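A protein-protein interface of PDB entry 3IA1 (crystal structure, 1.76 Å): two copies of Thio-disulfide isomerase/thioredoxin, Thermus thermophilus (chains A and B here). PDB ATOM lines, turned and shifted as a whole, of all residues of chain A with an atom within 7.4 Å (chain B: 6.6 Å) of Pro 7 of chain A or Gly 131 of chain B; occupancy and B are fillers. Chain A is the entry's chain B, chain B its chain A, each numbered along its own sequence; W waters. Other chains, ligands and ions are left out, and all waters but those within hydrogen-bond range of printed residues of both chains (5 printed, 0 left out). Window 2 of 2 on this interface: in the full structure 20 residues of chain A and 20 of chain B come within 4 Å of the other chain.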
ATOM      1  N   VAL A   5       7.947  18.349  -6.644  1.00  0.00           N
ATOM      2  CA  VAL A   5       7.626  16.898  -6.859  1.00  0.00           C
ATOM      3  C   VAL A   5       7.099  16.237  -5.572  1.00  0.00           C
ATOM      4  O   VAL A   5       7.818  15.499  -4.890  1.00  0.00           O
ATOM      5  CB  VAL A   5       8.831  16.110  -7.475  1.00  0.00           C
ATOM      6  CG1 VAL A   5       8.769  16.158  -8.998  1.00  0.00           C
ATOM      7  CG2 VAL A   5      10.173  16.679  -6.992  1.00  0.00           C
ATOM      8  N   LYS A   6       5.831  16.521  -5.260  1.00  0.00           N
ATOM      9  CA  LYS A   6       5.198  16.076  -4.010  1.00  0.00           C
ATOM     10  C   LYS A   6       4.855  14.586  -4.016  1.00  0.00           C
ATOM     11  O   LYS A   6       4.463  14.038  -5.050  1.00  0.00           O
ATOM     12  CB  LYS A   6       3.988  16.955  -3.651  1.00  0.00           C
ATOM     13  CG  LYS A   6       4.394  18.378  -3.235  1.00  0.00           C
ATOM     14  CD  LYS A   6       3.324  19.114  -2.428  1.00  0.00           C
ATOM     15  CE  LYS A   6       3.655  19.162  -0.933  1.00  0.00           C
ATOM     16  NZ  LYS A   6       3.180  17.970  -0.163  1.00  0.00           N
ATOM     17  N   PRO A   7       5.064  13.913  -2.869  1.00  0.00           N
ATOM     18  CA  PRO A   7       4.905  12.464  -2.772  1.00  0.00           C
ATOM     19  C   PRO A   7       3.514  11.892  -3.103  1.00  0.00           C
ATOM     20  O   PRO A   7       2.506  12.585  -3.009  1.00  0.00           O
ATOM     21  CB  PRO A   7       5.252  12.170  -1.308  1.00  0.00           C
ATOM     22  CG  PRO A   7       6.121  13.309  -0.895  1.00  0.00           C
ATOM     23  CD  PRO A   7       5.529  14.487  -1.591  1.00  0.00           C
ATOM     24  N   GLY A   8       3.498  10.624  -3.492  1.00  0.00           N
ATOM     25  CA  GLY A   8       2.261   9.857  -3.597  1.00  0.00           C
ATOM     26  C   GLY A   8       1.582   9.942  -4.940  1.00  0.00           C
ATOM     27  O   GLY A   8       2.206  10.306  -5.944  1.00  0.00           O
ATOM     28  N   GLU A   9       0.293   9.607  -4.951  1.00  0.00           N
ATOM     29  CA  GLU A   9      -0.515   9.611  -6.172  1.00  0.00           C
ATOM     30  C   GLU A   9      -1.901  10.195  -5.891  1.00  0.00           C
ATOM     31  O   GLU A   9      -2.472   9.926  -4.826  1.00  0.00           O
ATOM     32  CB  GLU A   9      -0.646   8.183  -6.744  1.00  0.00           C
ATOM     33  CG  GLU A   9       0.665   7.485  -7.129  1.00  0.00           C
ATOM     34  CD  GLU A   9       1.298   7.961  -8.436  1.00  0.00           C
ATOM     35  OE1 GLU A   9       1.274   9.171  -8.712  1.00  0.00           O
ATOM     36  OE2 GLU A   9       1.860   7.113  -9.173  1.00  0.00           O
ATOM     37  N   PRO A  10      -2.455  10.993  -6.836  1.00  0.00           N
ATOM     38  CA  PRO A  10      -3.833  11.494  -6.686  1.00  0.00           C
ATOM     39  C   PRO A  10      -4.831  10.347  -6.666  1.00  0.00           C
ATOM     40  O   PRO A  10      -4.584   9.279  -7.235  1.00  0.00           O
ATOM     41  CB  PRO A  10      -4.087  12.305  -7.982  1.00  0.00           C
ATOM     42  CG  PRO A  10      -2.760  12.492  -8.616  1.00  0.00           C
ATOM     43  CD  PRO A  10      -1.809  11.480  -8.077  1.00  0.00           C
ATOM     44  N   ASP A 117      -3.441  12.456   2.132  1.00  0.00           N
ATOM     45  CA  ASP A 117      -2.981  13.672   2.826  1.00  0.00           C
ATOM     46  C   ASP A 117      -3.934  14.872   2.622  1.00  0.00           C
ATOM     47  O   ASP A 117      -4.962  14.707   1.963  1.00  0.00           O
ATOM     48  CB  ASP A 117      -1.509  14.003   2.496  1.00  0.00           C
ATOM     49  CG  ASP A 117      -1.296  14.525   1.081  1.00  0.00           C
ATOM     50  OD1 ASP A 117      -2.256  14.743   0.314  1.00  0.00           O
ATOM     51  OD2 ASP A 117      -0.111  14.717   0.733  1.00  0.00           O
ATOM     52  N   GLU A 119      -3.831  17.300   0.662  1.00  0.00           N
ATOM     53  CA  GLU A 119      -3.955  17.672  -0.747  1.00  0.00           C
ATOM     54  C   GLU A 119      -4.576  16.559  -1.591  1.00  0.00           C
ATOM     55  O   GLU A 119      -4.613  16.643  -2.822  1.00  0.00           O
ATOM     56  CB  GLU A 119      -2.594  18.076  -1.325  1.00  0.00           C
ATOM     57  CG  GLU A 119      -2.083  19.424  -0.832  1.00  0.00           C
ATOM     58  CD  GLU A 119      -0.791  19.828  -1.515  1.00  0.00           C
ATOM     59  OE1 GLU A 119      -0.850  20.402  -2.624  1.00  0.00           O
ATOM     60  OE2 GLU A 119       0.287  19.562  -0.943  1.00  0.00           O
ATOM     61  N   LYS A 121      -3.640  13.312  -1.890  1.00  0.00           N
ATOM     62  CA  LYS A 121      -2.723  12.325  -2.438  1.00  0.00           C
ATOM     63  C   LYS A 121      -2.595  11.118  -1.515  1.00  0.00           C
ATOM     64  O   LYS A 121      -2.577  11.268  -0.297  1.00  0.00           O
ATOM     65  CB  LYS A 121      -1.340  12.943  -2.676  1.00  0.00           C
ATOM     66  CG  LYS A 121      -1.363  14.325  -3.348  1.00  0.00           C
ATOM     67  CD  LYS A 121      -2.174  14.325  -4.636  1.00  0.00           C
ATOM     68  CE  LYS A 121      -2.381  15.738  -5.168  1.00  0.00           C
ATOM     69  NZ  LYS A 121      -1.103  16.351  -5.594  1.00  0.00           N
ATOM     70  N   VAL A 122      -2.510   9.930  -2.120  1.00  0.00           N
ATOM     71  CA  VAL A 122      -2.263   8.683  -1.369  1.00  0.00           C
ATOM     72  C   VAL A 122      -0.758   8.629  -1.119  1.00  0.00           C
ATOM     73  O   VAL A 122       0.012   8.403  -2.052  1.00  0.00           O
ATOM     74  CB  VAL A 122      -2.736   7.448  -2.133  1.00  0.00           C
ATOM     75  CG1 VAL A 122      -2.342   6.165  -1.391  1.00  0.00           C
ATOM     76  CG2 VAL A 122      -4.269   7.512  -2.339  1.00  0.00           C
ATOM     77  N   VAL A 123      -0.357   8.844   0.133  1.00  0.00           N
ATOM     78  CA  VAL A 123       1.054   8.989   0.520  1.00  0.00           C
ATOM     79  C   VAL A 123       1.616   7.783   1.289  1.00  0.00           C
ATOM     80  O   VAL A 123       2.813   7.739   1.597  1.00  0.00           O
ATOM     81  CB  VAL A 123       1.289  10.268   1.361  1.00  0.00           C
ATOM     82  CG1 VAL A 123       1.129  11.542   0.490  1.00  0.00           C
ATOM     83  CG2 VAL A 123       0.332  10.333   2.589  1.00  0.00           C
ATOM     84  N   LEU A 141       2.637  12.354   9.143  1.00  0.00           N
ATOM     85  CA  LEU A 141       3.264  12.927   7.942  1.00  0.00           C
ATOM     86  C   LEU A 141       2.268  13.446   6.899  1.00  0.00           C
ATOM     87  O   LEU A 141       2.582  14.381   6.165  1.00  0.00           O
ATOM     88  CB  LEU A 141       4.253  11.956   7.305  1.00  0.00           C
ATOM     89  CG  LEU A 141       5.408  11.501   8.195  1.00  0.00           C
ATOM     90  CD1 LEU A 141       6.196  10.422   7.482  1.00  0.00           C
ATOM     91  CD2 LEU A 141       6.302  12.663   8.593  1.00  0.00           C
ATOM     92  N   VAL B  55      18.659   7.442   0.314  1.00  0.00           N
ATOM     93  CA  VAL B  55      18.178   6.643   1.428  1.00  0.00           C
ATOM     94  C   VAL B  55      18.940   5.322   1.536  1.00  0.00           C
ATOM     95  O   VAL B  55      19.331   4.917   2.633  1.00  0.00           O
ATOM     96  CB  VAL B  55      16.662   6.406   1.343  1.00  0.00           C
ATOM     97  CG1 VAL B  55      16.181   5.492   2.500  1.00  0.00           C
ATOM     98  CG2 VAL B  55      15.944   7.736   1.416  1.00  0.00           C
ATOM     99  N   PHE B 126       4.645   2.456  -1.189  1.00  0.00           N
ATOM    100  CA  PHE B 126       4.462   3.824  -1.667  1.00  0.00           C
ATOM    101  C   PHE B 126       4.291   3.752  -3.162  1.00  0.00           C
ATOM    102  O   PHE B 126       5.030   3.060  -3.828  1.00  0.00           O
ATOM    103  CB  PHE B 126       5.702   4.683  -1.329  1.00  0.00           C
ATOM    104  CG  PHE B 126       6.010   4.724   0.136  1.00  0.00           C
ATOM    105  CD1 PHE B 126       5.271   5.542   0.989  1.00  0.00           C
ATOM    106  CD2 PHE B 126       6.976   3.877   0.675  1.00  0.00           C
ATOM    107  CE1 PHE B 126       5.549   5.550   2.372  1.00  0.00           C
ATOM    108  CE2 PHE B 126       7.260   3.879   2.055  1.00  0.00           C
ATOM    109  CZ  PHE B 126       6.545   4.704   2.894  1.00  0.00           C
ATOM    110  N   ALA B 127       3.280   4.448  -3.667  1.00  0.00           N
ATOM    111  CA  ALA B 127       3.014   4.519  -5.089  1.00  0.00           C
ATOM    112  C   ALA B 127       3.551   5.859  -5.569  1.00  0.00           C
ATOM    113  O   ALA B 127       3.364   6.864  -4.905  1.00  0.00           O
ATOM    114  CB  ALA B 127       1.492   4.394  -5.362  1.00  0.00           C
ATOM    115  N   GLY B 128       4.214   5.866  -6.720  1.00  0.00           N
ATOM    116  CA  GLY B 128       4.731   7.112  -7.298  1.00  0.00           C
ATOM    117  C   GLY B 128       5.937   7.554  -6.501  1.00  0.00           C
ATOM    118  O   GLY B 128       6.727   6.717  -6.075  1.00  0.00           O
ATOM    119  N   ARG B 129       6.073   8.857  -6.263  1.00  0.00           N
ATOM    120  CA  ARG B 129       7.189   9.369  -5.475  1.00  0.00           C
ATOM    121  C   ARG B 129       6.997   9.049  -3.984  1.00  0.00           C
ATOM    122  O   ARG B 129       5.977   9.393  -3.387  1.00  0.00           O
ATOM    123  CB  ARG B 129       7.368  10.877  -5.732  1.00  0.00           C
ATOM    124  CG  ARG B 129       7.357  11.244  -7.234  1.00  0.00           C
ATOM    125  CD  ARG B 129       7.009  12.705  -7.502  1.00  0.00           C
ATOM    126  NE  ARG B 129       7.321  13.073  -8.885  1.00  0.00           N
ATOM    127  CZ  ARG B 129       6.443  13.122  -9.890  1.00  0.00           C
ATOM    128  NH1 ARG B 129       6.857  13.470 -11.103  1.00  0.00           N
ATOM    129  NH2 ARG B 129       5.155  12.833  -9.697  1.00  0.00           N
ATOM    130  N   ALA B 130       7.960   8.350  -3.393  1.00  0.00           N
ATOM    131  CA  ALA B 130       7.878   8.036  -1.976  1.00  0.00           C
ATOM    132  C   ALA B 130       8.427   9.240  -1.244  1.00  0.00           C
ATOM    133  O   ALA B 130       9.368   9.886  -1.720  1.00  0.00           O
ATOM    134  CB  ALA B 130       8.678   6.799  -1.625  1.00  0.00           C
ATOM    135  N   GLY B 131       7.858   9.554  -0.092  1.00  0.00           N
ATOM    136  CA  GLY B 131       8.404  10.666   0.686  1.00  0.00           C
ATOM    137  C   GLY B 131       9.755  10.297   1.279  1.00  0.00           C
ATOM    138  O   GLY B 131       9.959   9.163   1.701  1.00  0.00           O
ATOM    139  N   ARG B 132      10.695  11.238   1.300  1.00  0.00           N
ATOM    140  CA  ARG B 132      11.977  10.976   1.949  1.00  0.00           C
ATOM    141  C   ARG B 132      11.804  10.627   3.447  1.00  0.00           C
ATOM    142  O   ARG B 132      12.294   9.595   3.935  1.00  0.00           O
ATOM    143  CB  ARG B 132      12.911  12.178   1.786  1.00  0.00           C
ATOM    144  CG  ARG B 132      14.180  12.013   2.557  1.00  0.00           C
ATOM    145  CD  ARG B 132      15.203  13.117   2.283  1.00  0.00           C
ATOM    146  NE  ARG B 132      16.167  13.139   3.381  1.00  0.00           N
ATOM    147  CZ  ARG B 132      17.160  12.270   3.542  1.00  0.00           C
ATOM    148  NH1 ARG B 132      17.373  11.316   2.641  1.00  0.00           N
ATOM    149  NH2 ARG B 132      17.949  12.368   4.611  1.00  0.00           N
ATOM    150  N   GLU B 133      11.091  11.488   4.169  1.00  0.00           N
ATOM    151  CA  GLU B 133      10.854  11.254   5.580  1.00  0.00           C
ATOM    152  C   GLU B 133       9.999   9.997   5.780  1.00  0.00           C
ATOM    153  O   GLU B 133      10.290   9.193   6.666  1.00  0.00           O
ATOM    154  CB  GLU B 133      10.200  12.474   6.225  1.00  0.00           C
ATOM    155  CG  GLU B 133      10.166  12.389   7.744  1.00  0.00           C
ATOM    156  CD  GLU B 133       9.667  13.669   8.399  1.00  0.00           C
ATOM    157  OE1 GLU B 133       9.239  14.590   7.673  1.00  0.00           O
ATOM    158  OE2 GLU B 133       9.686  13.738   9.646  1.00  0.00           O
ATOM    159  N   ALA B 134       8.978   9.836   4.938  1.00  0.00           N
ATOM    160  CA  ALA B 134       8.095   8.654   4.980  1.00  0.00           C
ATOM    161  C   ALA B 134       8.876   7.349   4.851  1.00  0.00           C
ATOM    162  O   ALA B 134       8.693   6.422   5.654  1.00  0.00           O
ATOM    163  CB  ALA B 134       7.024   8.744   3.891  1.00  0.00           C
ATOM    164  N   LEU B 135       9.744   7.288   3.842  1.00  0.00           N
ATOM    165  CA  LEU B 135      10.559   6.090   3.586  1.00  0.00           C
ATOM    166  C   LEU B 135      11.544   5.832   4.725  1.00  0.00           C
ATOM    167  O   LEU B 135      11.648   4.700   5.187  1.00  0.00           O
ATOM    168  CB  LEU B 135      11.278   6.181   2.238  1.00  0.00           C
ATOM    169  CG  LEU B 135      12.090   4.933   1.845  1.00  0.00           C
ATOM    170  CD1 LEU B 135      11.194   3.670   1.858  1.00  0.00           C
ATOM    171  CD2 LEU B 135      12.734   5.099   0.459  1.00  0.00           C
ATOM    172  N   LEU B 136      12.230   6.876   5.204  1.00  0.00           N
ATOM    173  CA  LEU B 136      13.164   6.707   6.323  1.00  0.00           C
ATOM    174  C   LEU B 136      12.433   6.213   7.562  1.00  0.00           C
ATOM    175  O   LEU B 136      12.877   5.271   8.199  1.00  0.00           O
ATOM    176  CB  LEU B 136      13.913   8.014   6.639  1.00  0.00           C
ATOM    177  CG  LEU B 136      15.064   8.338   5.683  1.00  0.00           C
ATOM    178  CD1 LEU B 136      15.456   9.820   5.778  1.00  0.00           C
ATOM    179  CD2 LEU B 136      16.245   7.450   5.946  1.00  0.00           C
HETATM  180  O   HOH W   1       4.173   8.111  -1.505  1.00  0.00           O
HETATM  181  O   HOH W   2       4.557  10.767  -6.685  1.00  0.00           O
HETATM  182  O   HOH W   3       2.108   6.440  -1.896  1.00  0.00           O
HETATM  183  O   HOH W   4       2.568   4.151  -9.089  1.00  0.00           O
HETATM  184  O   HOH W   5       4.967   9.410   0.745  1.00  0.00           O
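N of Gly 8 of chain A is in hydrogen-bond range of O of Arg 129 of chain B, at 2.8 Å.
OE2 of Glu 119 of chain A lies within salt-bridge range of NZ of Lys 6 of chain A (3.4 Å). The backbone carbonyl oxygen (O) of Glu 9 of chain A lies within hydrogen-bond range of the backbone NH (N) of Val 122 of chain A.
Among the printed residues, merely in contact across the chains: Pro 7 of chain A with Arg 129 of chain B (3.3 Å), Val 123 of chain A with Phe 126 of chain B (3.4 Å), Val 5 of chain A with Arg 129 of chain B (3.4 Å), Glu 9 of chain A with Gly 128 of chain B (3.4 Å), Gly 8 of chain A with Ala 127 of chain B (3.4 Å), Leu 141 of chain A with Glu 133 of chain B (3.5 Å), Glu 9 of chain A with Ala 127 of chain B (3.6 Å), Leu 141 of chain A with Ala 134 of chain B (3.6 Å), Lys 6 of chain A with Arg 129 of chain B (3.8 Å) and Pro 7 of chain A with Gly 131 of chain B (3.8 Å).
Of the printed residues of chain B, Pro 7 of chain A touches Arg 129 and Gly 131. Of the printed residues of chain A, Ala 127 of chain B touches Gly 8 (3.4 Å) and Glu 9 (3.6 Å). Of the printed residues of chain A, Ala 134 of chain B touches Leu 141 (3.6 Å). The nearest printed residue of chain B that does not touch Pro 7 of chain A is Ala 130 of chain B (4.3 Å). The nearest printed residue of chain A that does not touch Gly 131 of chain B is Val 123 of chain A (5.6 Å).
Of the 12 printed residues of chain B, 7 touch a printed residue of chain A. Printed residues of chain B that touch a printed residue of chain A: Phe 126, Ala 127, Gly 128, Arg 129, Gly 131, Glu 133 and Ala 134. Hydrophobic or aromatic side chains of chain A that line the printed part of chain B: Val 5, Pro 7 and Leu 141. Among the printed residues, no Asp or Glu carboxylate lies within 4 Å of a Lys or Arg side-chain nitrogen of the other chain.
No position is printed for both chains.
Water W2 lies within hydrogen-bond range of the backbone NH of Arg 129 of chain B (2.5 Å) and the backbone carbonyl oxygen of Gly 8 of chain A (2.5 Å). Water W5 bridges O of Val 123 of chain A and N of Gly 131 of chain B. Water W3 lies within hydrogen-bond range of O of Val 122 of chain A and N of Ala 127 of chain B. Water W1 lies within hydrogen-bond range of the backbone carbonyl oxygen of Arg 129 of chain B, the backbone NH of Gly 8 of chain A and the backbone carbonyl oxygen of Val 123 of chain A. Water W4 lies within hydrogen-bond range of the side-chain carboxylate of Glu 9 of chain A (3.0 Å) and the backbone NH of Gly 128 of chain B (3.4 Å).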
